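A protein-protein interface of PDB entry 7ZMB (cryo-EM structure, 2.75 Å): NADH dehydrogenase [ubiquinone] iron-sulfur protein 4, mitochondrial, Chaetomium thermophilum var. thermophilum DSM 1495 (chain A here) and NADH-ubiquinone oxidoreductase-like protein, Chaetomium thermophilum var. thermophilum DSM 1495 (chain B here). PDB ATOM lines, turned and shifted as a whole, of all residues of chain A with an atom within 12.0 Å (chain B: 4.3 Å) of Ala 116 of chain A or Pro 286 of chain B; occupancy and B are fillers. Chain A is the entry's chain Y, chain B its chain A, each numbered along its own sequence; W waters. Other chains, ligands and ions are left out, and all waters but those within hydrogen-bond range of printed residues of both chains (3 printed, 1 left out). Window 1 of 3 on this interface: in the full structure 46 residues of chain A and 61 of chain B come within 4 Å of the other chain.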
ATOM      1  N   LYS A 111       6.381 -26.086  -8.574  1.00  0.00           N
ATOM      2  CA  LYS A 111       6.553 -27.175  -7.629  1.00  0.00           C
ATOM      3  C   LYS A 111       6.449 -26.611  -6.228  1.00  0.00           C
ATOM      4  O   LYS A 111       7.271 -25.761  -5.861  1.00  0.00           O
ATOM      5  CB  LYS A 111       7.899 -27.864  -7.813  1.00  0.00           C
ATOM      6  CG  LYS A 111       8.024 -28.622  -9.101  1.00  0.00           C
ATOM      7  CD  LYS A 111       9.386 -29.227  -9.258  1.00  0.00           C
ATOM      8  CE  LYS A 111       9.582 -30.386  -8.328  1.00  0.00           C
ATOM      9  NZ  LYS A 111       8.712 -31.510  -8.737  1.00  0.00           N
ATOM     10  N   PRO A 112       5.471 -27.022  -5.430  1.00  0.00           N
ATOM     11  CA  PRO A 112       5.344 -26.473  -4.079  1.00  0.00           C
ATOM     12  C   PRO A 112       6.616 -26.686  -3.276  1.00  0.00           C
ATOM     13  O   PRO A 112       7.216 -27.760  -3.305  1.00  0.00           O
ATOM     14  CB  PRO A 112       4.167 -27.257  -3.500  1.00  0.00           C
ATOM     15  CG  PRO A 112       3.373 -27.611  -4.690  1.00  0.00           C
ATOM     16  CD  PRO A 112       4.383 -27.962  -5.725  1.00  0.00           C
ATOM     17  N   ALA A 113       7.032 -25.643  -2.570  1.00  0.00           N
ATOM     18  CA  ALA A 113       8.204 -25.752  -1.726  1.00  0.00           C
ATOM     19  C   ALA A 113       7.866 -26.543  -0.468  1.00  0.00           C
ATOM     20  O   ALA A 113       6.709 -26.654  -0.062  1.00  0.00           O
ATOM     21  CB  ALA A 113       8.740 -24.370  -1.362  1.00  0.00           C
ATOM     22  N   LYS A 114       8.901 -27.111   0.135  1.00  0.00           N
ATOM     23  CA  LYS A 114       8.728 -27.840   1.374  1.00  0.00           C
ATOM     24  C   LYS A 114       8.203 -26.904   2.456  1.00  0.00           C
ATOM     25  O   LYS A 114       8.670 -25.768   2.577  1.00  0.00           O
ATOM     26  CB  LYS A 114      10.053 -28.462   1.807  1.00  0.00           C
ATOM     27  CG  LYS A 114      10.004 -29.238   3.101  1.00  0.00           C
ATOM     28  CD  LYS A 114      11.392 -29.446   3.662  1.00  0.00           C
ATOM     29  CE  LYS A 114      11.863 -28.233   4.423  1.00  0.00           C
ATOM     30  NZ  LYS A 114      11.003 -27.918   5.589  1.00  0.00           N
ATOM     31  N   PRO A 115       7.219 -27.334   3.239  1.00  0.00           N
ATOM     32  CA  PRO A 115       6.792 -26.532   4.387  1.00  0.00           C
ATOM     33  C   PRO A 115       7.938 -26.328   5.366  1.00  0.00           C
ATOM     34  O   PRO A 115       8.796 -27.193   5.542  1.00  0.00           O
ATOM     35  CB  PRO A 115       5.671 -27.373   5.003  1.00  0.00           C
ATOM     36  CG  PRO A 115       5.948 -28.772   4.514  1.00  0.00           C
ATOM     37  CD  PRO A 115       6.471 -28.600   3.140  1.00  0.00           C
ATOM     38  N   ALA A 116       7.961 -25.152   5.991  1.00  0.00           N
ATOM     39  CA  ALA A 116       9.010 -24.865   6.960  1.00  0.00           C
ATOM     40  C   ALA A 116       8.889 -25.746   8.190  1.00  0.00           C
ATOM     41  O   ALA A 116       9.887 -26.013   8.863  1.00  0.00           O
ATOM     42  CB  ALA A 116       8.966 -23.394   7.361  1.00  0.00           C
ATOM     43  N   THR A 117       7.687 -26.223   8.480  1.00  0.00           N
ATOM     44  CA  THR A 117       7.395 -26.893   9.732  1.00  0.00           C
ATOM     45  C   THR A 117       7.707 -28.380   9.719  1.00  0.00           C
ATOM     46  O   THR A 117       7.669 -29.005  10.780  1.00  0.00           O
ATOM     47  CB  THR A 117       5.923 -26.682  10.099  1.00  0.00           C
ATOM     48  OG1 THR A 117       5.088 -27.281   9.099  1.00  0.00           O
ATOM     49  CG2 THR A 117       5.619 -25.208  10.182  1.00  0.00           C
ATOM     50  N   GLN A 118       8.019 -28.963   8.567  1.00  0.00           N
ATOM     51  CA  GLN A 118       8.261 -30.392   8.471  1.00  0.00           C
ATOM     52  C   GLN A 118       9.496 -30.656   7.627  1.00  0.00           C
ATOM     53  O   GLN A 118       9.943 -29.803   6.863  1.00  0.00           O
ATOM     54  CB  GLN A 118       7.058 -31.124   7.879  1.00  0.00           C
ATOM     55  CG  GLN A 118       5.801 -30.983   8.706  1.00  0.00           C
ATOM     56  CD  GLN A 118       4.910 -32.180   8.610  1.00  0.00           C
ATOM     57  OE1 GLN A 118       3.809 -32.099   8.088  1.00  0.00           O
ATOM     58  NE2 GLN A 118       5.386 -33.307   9.092  1.00  0.00           N
ATOM     59  N   SER A 119      10.051 -31.855   7.784  1.00  0.00           N
ATOM     60  CA  SER A 119      11.189 -32.302   6.995  1.00  0.00           C
ATOM     61  C   SER A 119      10.801 -33.245   5.866  1.00  0.00           C
ATOM     62  O   SER A 119      11.623 -33.491   4.982  1.00  0.00           O
ATOM     63  CB  SER A 119      12.227 -32.988   7.894  1.00  0.00           C
ATOM     64  OG  SER A 119      12.933 -32.041   8.667  1.00  0.00           O
ATOM     65  N   GLY A 120       9.586 -33.785   5.879  1.00  0.00           N
ATOM     66  CA  GLY A 120       9.133 -34.604   4.771  1.00  0.00           C
ATOM     67  C   GLY A 120       8.915 -33.772   3.521  1.00  0.00           C
ATOM     68  O   GLY A 120       8.513 -32.611   3.581  1.00  0.00           O
ATOM     69  N   GLU A 121       9.168 -34.391   2.369  1.00  0.00           N
ATOM     70  CA  GLU A 121       9.248 -33.684   1.097  1.00  0.00           C
ATOM     71  C   GLU A 121       8.358 -34.296   0.020  1.00  0.00           C
ATOM     72  O   GLU A 121       8.617 -34.103  -1.166  1.00  0.00           O
ATOM     73  CB  GLU A 121      10.701 -33.645   0.629  1.00  0.00           C
ATOM     74  CG  GLU A 121      11.646 -33.099   1.681  1.00  0.00           C
ATOM     75  CD  GLU A 121      12.905 -32.488   1.102  1.00  0.00           C
ATOM     76  OE1 GLU A 121      13.522 -33.116   0.216  1.00  0.00           O
ATOM     77  OE2 GLU A 121      13.280 -31.382   1.539  1.00  0.00           O
ATOM     78  N   LYS A 122       7.299 -35.003   0.401  1.00  0.00           N
ATOM     79  CA  LYS A 122       6.469 -35.708  -0.614  1.00  0.00           C
ATOM     80  C   LYS A 122       5.568 -34.736  -1.392  1.00  0.00           C
ATOM     81  O   LYS A 122       5.149 -35.100  -2.503  1.00  0.00           O
ATOM     82  CB  LYS A 122       5.669 -36.834   0.040  1.00  0.00           C
ATOM     83  CG  LYS A 122       5.420 -38.031  -0.864  1.00  0.00           C
ATOM     84  CD  LYS A 122       3.974 -38.424  -0.872  1.00  0.00           C
ATOM     85  CE  LYS A 122       3.341 -38.165   0.474  1.00  0.00           C
ATOM     86  NZ  LYS A 122       1.967 -38.707   0.552  1.00  0.00           N
ATOM     87  N   ASN A 123       5.281 -33.555  -0.850  1.00  0.00           N
ATOM     88  CA  ASN A 123       4.337 -32.616  -1.507  1.00  0.00           C
ATOM     89  C   ASN A 123       5.170 -31.731  -2.430  1.00  0.00           C
ATOM     90  O   ASN A 123       4.585 -30.908  -3.158  1.00  0.00           O
ATOM     91  CB  ASN A 123       3.389 -31.961  -0.499  1.00  0.00           C
ATOM     92  CG  ASN A 123       2.723 -32.966   0.419  1.00  0.00           C
ATOM     93  OD1 ASN A 123       2.717 -34.161   0.140  1.00  0.00           O
ATOM     94  ND2 ASN A 123       2.155 -32.499   1.516  1.00  0.00           N
ATOM     95  N   THR A 124       6.492 -31.925  -2.418  1.00  0.00           N
ATOM     96  CA  THR A 124       7.370 -31.228  -3.348  1.00  0.00           C
ATOM     97  C   THR A 124       7.660 -32.035  -4.605  1.00  0.00           C
ATOM     98  O   THR A 124       8.397 -31.557  -5.468  1.00  0.00           O
ATOM     99  CB  THR A 124       8.698 -30.870  -2.664  1.00  0.00           C
ATOM    100  OG1 THR A 124       9.489 -32.049  -2.492  1.00  0.00           O
ATOM    101  CG2 THR A 124       8.459 -30.240  -1.319  1.00  0.00           C
ATOM    102  N   GLN A 181       6.922 -20.486 -12.220  1.00  0.00           N
ATOM    103  CA  GLN A 181       8.066 -20.137 -11.397  1.00  0.00           C
ATOM    104  C   GLN A 181       8.929 -21.377 -11.245  1.00  0.00           C
ATOM    105  O   GLN A 181       8.412 -22.493 -11.174  1.00  0.00           O
ATOM    106  CB  GLN A 181       7.674 -19.590 -10.022  1.00  0.00           C
ATOM    107  CG  GLN A 181       6.992 -20.528  -9.096  1.00  0.00           C
ATOM    108  CD  GLN A 181       6.612 -19.844  -7.807  1.00  0.00           C
ATOM    109  OE1 GLN A 181       6.913 -18.670  -7.613  1.00  0.00           O
ATOM    110  NE2 GLN A 181       5.986 -20.583  -6.900  1.00  0.00           N
ATOM    111  N   ASN A 184      13.370 -23.187  -6.317  1.00  0.00           N
ATOM    112  CA  ASN A 184      14.688 -22.836  -5.811  1.00  0.00           C
ATOM    113  C   ASN A 184      15.358 -24.108  -5.317  1.00  0.00           C
ATOM    114  O   ASN A 184      14.792 -24.835  -4.495  1.00  0.00           O
ATOM    115  CB  ASN A 184      14.601 -21.803  -4.691  1.00  0.00           C
ATOM    116  CG  ASN A 184      13.692 -20.653  -5.027  1.00  0.00           C
ATOM    117  OD1 ASN A 184      13.657 -20.190  -6.160  1.00  0.00           O
ATOM    118  ND2 ASN A 184      12.942 -20.189  -4.044  1.00  0.00           N
ATOM    119  N   ARG A 186      18.336 -26.448  -3.519  1.00  0.00           N
ATOM    120  CA  ARG A 186      19.267 -26.454  -2.404  1.00  0.00           C
ATOM    121  C   ARG A 186      20.699 -26.382  -2.912  1.00  0.00           C
ATOM    122  O   ARG A 186      21.071 -27.070  -3.865  1.00  0.00           O
ATOM    123  CB  ARG A 186      19.047 -27.732  -1.600  1.00  0.00           C
ATOM    124  CG  ARG A 186      17.698 -27.771  -0.922  1.00  0.00           C
ATOM    125  CD  ARG A 186      17.449 -29.058  -0.165  1.00  0.00           C
ATOM    126  NE  ARG A 186      18.302 -29.292   0.989  1.00  0.00           N
ATOM    127  CZ  ARG A 186      18.309 -30.447   1.644  1.00  0.00           C
ATOM    128  NH1 ARG A 186      17.508 -31.429   1.255  1.00  0.00           N
ATOM    129  NH2 ARG A 186      19.102 -30.629   2.677  1.00  0.00           N
ATOM    130  N   ASP B 235       9.620 -22.851  13.799  1.00  0.00           N
ATOM    131  CA  ASP B 235       9.557 -23.741  12.649  1.00  0.00           C
ATOM    132  C   ASP B 235      10.574 -24.864  12.742  1.00  0.00           C
ATOM    133  O   ASP B 235      10.309 -25.970  12.266  1.00  0.00           O
ATOM    134  CB  ASP B 235       9.756 -22.948  11.364  1.00  0.00           C
ATOM    135  CG  ASP B 235       8.610 -22.003  11.092  1.00  0.00           C
ATOM    136  OD1 ASP B 235       7.444 -22.399  11.307  1.00  0.00           O
ATOM    137  OD2 ASP B 235       8.873 -20.864  10.668  1.00  0.00           O
ATOM    138  N   ASN B 271      11.927 -14.970   0.591  1.00  0.00           N
ATOM    139  CA  ASN B 271      10.870 -15.803   0.041  1.00  0.00           C
ATOM    140  C   ASN B 271      10.038 -16.387   1.169  1.00  0.00           C
ATOM    141  O   ASN B 271      10.569 -17.014   2.088  1.00  0.00           O
ATOM    142  CB  ASN B 271      11.465 -16.903  -0.825  1.00  0.00           C
ATOM    143  CG  ASN B 271      12.131 -16.360  -2.061  1.00  0.00           C
ATOM    144  OD1 ASN B 271      12.690 -15.266  -2.052  1.00  0.00           O
ATOM    145  ND2 ASN B 271      12.034 -17.101  -3.149  1.00  0.00           N
ATOM    146  N   LEU B 285       5.376 -17.971   6.831  1.00  0.00           N
ATOM    147  CA  LEU B 285       6.443 -18.948   6.954  1.00  0.00           C
ATOM    148  C   LEU B 285       7.567 -18.649   5.973  1.00  0.00           C
ATOM    149  O   LEU B 285       7.335 -18.093   4.899  1.00  0.00           O
ATOM    150  CB  LEU B 285       5.946 -20.374   6.693  1.00  0.00           C
ATOM    151  CG  LEU B 285       5.073 -21.108   7.713  1.00  0.00           C
ATOM    152  CD1 LEU B 285       5.067 -22.578   7.401  1.00  0.00           C
ATOM    153  CD2 LEU B 285       5.542 -20.870   9.130  1.00  0.00           C
ATOM    154  N   PRO B 286       8.798 -19.006   6.312  1.00  0.00           N
ATOM    155  CA  PRO B 286       9.871 -18.955   5.319  1.00  0.00           C
ATOM    156  C   PRO B 286       9.783 -20.124   4.359  1.00  0.00           C
ATOM    157  O   PRO B 286       9.275 -21.198   4.691  1.00  0.00           O
ATOM    158  CB  PRO B 286      11.137 -19.038   6.173  1.00  0.00           C
ATOM    159  CG  PRO B 286      10.704 -19.773   7.368  1.00  0.00           C
ATOM    160  CD  PRO B 286       9.315 -19.330   7.648  1.00  0.00           C
ATOM    161  N   ARG B 287      10.289 -19.911   3.157  1.00  0.00           N
ATOM    162  CA  ARG B 287      10.495 -20.996   2.217  1.00  0.00           C
ATOM    163  C   ARG B 287      11.886 -20.877   1.618  1.00  0.00           C
ATOM    164  O   ARG B 287      12.494 -19.810   1.626  1.00  0.00           O
ATOM    165  CB  ARG B 287       9.434 -21.014   1.123  1.00  0.00           C
ATOM    166  CG  ARG B 287       9.407 -19.813   0.255  1.00  0.00           C
ATOM    167  CD  ARG B 287       8.337 -19.949  -0.789  1.00  0.00           C
ATOM    168  NE  ARG B 287       8.107 -18.678  -1.456  1.00  0.00           N
ATOM    169  CZ  ARG B 287       8.632 -18.339  -2.622  1.00  0.00           C
ATOM    170  NH1 ARG B 287       9.414 -19.186  -3.264  1.00  0.00           N
ATOM    171  NH2 ARG B 287       8.369 -17.153  -3.139  1.00  0.00           N
ATOM    172  N   GLU B 295      16.137 -20.244   4.147  1.00  0.00           N
ATOM    173  CA  GLU B 295      15.135 -20.838   5.030  1.00  0.00           C
ATOM    174  C   GLU B 295      14.860 -20.021   6.289  1.00  0.00           C
ATOM    175  O   GLU B 295      14.117 -20.492   7.149  1.00  0.00           O
ATOM    176  CB  GLU B 295      15.499 -22.272   5.449  1.00  0.00           C
ATOM    177  CG  GLU B 295      15.259 -23.315   4.377  1.00  0.00           C
ATOM    178  CD  GLU B 295      16.008 -24.615   4.616  1.00  0.00           C
ATOM    179  OE1 GLU B 295      17.061 -24.818   3.980  1.00  0.00           O
ATOM    180  OE2 GLU B 295      15.538 -25.452   5.411  1.00  0.00           O
ATOM    181  N   TRP B 296      15.405 -18.816   6.423  1.00  0.00           N
ATOM    182  CA  TRP B 296      15.161 -17.976   7.588  1.00  0.00           C
ATOM    183  C   TRP B 296      14.451 -16.691   7.190  1.00  0.00           C
ATOM    184  O   TRP B 296      14.699 -16.141   6.114  1.00  0.00           O
ATOM    185  CB  TRP B 296      16.456 -17.610   8.314  1.00  0.00           C
ATOM    186  CG  TRP B 296      17.466 -18.696   8.415  1.00  0.00           C
ATOM    187  CD1 TRP B 296      18.764 -18.630   8.033  1.00  0.00           C
ATOM    188  CD2 TRP B 296      17.274 -20.007   8.953  1.00  0.00           C
ATOM    189  NE1 TRP B 296      19.393 -19.811   8.291  1.00  0.00           N
ATOM    190  CE2 TRP B 296      18.498 -20.676   8.855  1.00  0.00           C
ATOM    191  CE3 TRP B 296      16.181 -20.678   9.507  1.00  0.00           C
ATOM    192  CZ2 TRP B 296      18.664 -21.982   9.287  1.00  0.00           C
ATOM    193  CZ3 TRP B 296      16.346 -21.967   9.923  1.00  0.00           C
ATOM    194  CH2 TRP B 296      17.578 -22.608   9.818  1.00  0.00           C
ATOM    195  N   ILE B 297      13.560 -16.225   8.064  1.00  0.00           N
ATOM    196  CA  ILE B 297      12.995 -14.886   8.005  1.00  0.00           C
ATOM    197  C   ILE B 297      13.160 -14.269   9.382  1.00  0.00           C
ATOM    198  O   ILE B 297      13.319 -14.972  10.379  1.00  0.00           O
ATOM    199  CB  ILE B 297      11.513 -14.875   7.575  1.00  0.00           C
ATOM    200  CG1 ILE B 297      10.657 -15.731   8.516  1.00  0.00           C
ATOM    201  CG2 ILE B 297      11.381 -15.332   6.135  1.00  0.00           C
ATOM    202  CD1 ILE B 297       9.181 -15.634   8.264  1.00  0.00           C
ATOM    203  N   ARG B 302       8.079 -12.085   9.961  1.00  0.00           N
ATOM    204  CA  ARG B 302       7.223 -13.180  10.396  1.00  0.00           C
ATOM    205  C   ARG B 302       5.958 -12.672  11.078  1.00  0.00           C
ATOM    206  O   ARG B 302       4.843 -13.005  10.669  1.00  0.00           O
ATOM    207  CB  ARG B 302       8.009 -14.092  11.342  1.00  0.00           C
ATOM    208  CG  ARG B 302       7.366 -15.421  11.615  1.00  0.00           C
ATOM    209  CD  ARG B 302       8.180 -16.228  12.587  1.00  0.00           C
ATOM    210  NE  ARG B 302       9.336 -16.845  11.963  1.00  0.00           N
ATOM    211  CZ  ARG B 302       9.300 -17.983  11.285  1.00  0.00           C
ATOM    212  NH1 ARG B 302       8.159 -18.634  11.138  1.00  0.00           N
ATOM    213  NH2 ARG B 302      10.407 -18.472  10.758  1.00  0.00           N
HETATM  214  O   HOH W   1       7.243 -22.504   4.122  1.00  0.00           O
HETATM  215  O   HOH W   2       8.068 -16.015  -6.376  1.00  0.00           O
HETATM  216  O   HOH W   3      10.795 -21.942  -2.276  1.00  0.00           O
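The side-chain amide nitrogen of Asn 184 of chain A lies close to the side-chain amide nitrogen of Asn 271 of chain B (3.3 Å).
The backbone carbonyl oxygen (O) of Asp 235 of chain B sits close to the backbone carbonyl oxygen (O) of Ala 116 of chain A (3.4 Å).
The guanidinium group (NH2) of Arg 302 of chain B lies within salt-bridge range of the side-chain carboxylate (OD2) of Asp 235 of chain B, 2.8 Å away.
N of Arg 287 of chain B sits at hydrogen-bond distance from O of Asn 271 of chain B, 3.1 Å away.
CD1 of Leu 285 of chain B touches CB of Ala 116 of chain A, 3.98 Å away.
Pro 286 of chain B touches Ala 116 of chain A.
Asp 235 of chain B touches Thr 117 of chain A (OD1 to CG2, 3.5 Å).
Leu 285 of chain B touches Thr 117 of chain A (CD1 to CG2, 3.9 Å).
ND2 of Asn 184 of chain A touches NH1 of Arg 287 of chain B (3.7 Å).
Of the printed residues of chain B, Ala 116 of chain A touches Asp 235, Leu 285 and Pro 286.
Of the printed residues of chain A, Asp 235 of chain B touches Ala 116 (3.4 Å) and Thr 117 (3.5 Å).
Printed residues of chain A within 4 Å of Asn 271 of chain B: Asn 184 (3.3 Å).
Of chain A, only Ala 116 (3.5 Å) comes within 4 Å of Pro 286 of chain B.
Printed residues of chain A within 4 Å of Arg 287 of chain B: Asn 184.
No residue of chain A comes within 4 Å of Ile 297 of chain B.
The nearest residue of chain A that does not touch Pro 286 of chain B is Lys 114 of chain A (5.1 Å).
Hydrophobic or aromatic side chains of chain B that line the printed part of chain A: Leu 285.
Of the 17 printed residues of chain A, 3 touch a printed residue of chain B.
Printed residues of chain A that touch a printed residue of chain B: Ala 116, Thr 117 and Asn 184.
Along chain A the printed residues that touch a printed residue of chain B span positions 116 to 184.
Among the printed residues, 7 pairs touch across the chains.
Water W1 lies within hydrogen-bond range of the backbone carbonyl oxygen (O) of Pro 286 of chain B (2.5 Å) and the backbone NH (N) of Ala 116 of chain A (3.3 Å).
Water W2 bridges OE1 of Gln 181 of chain A (3.1 Å) and NH2 of Arg 287 of chain B (3.4 Å).
Water W3 lies within hydrogen-bond range of NH1 of Arg 287 of chain B (3.2 Å) and ND2 of Asn 184 of chain A (3.3 Å).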
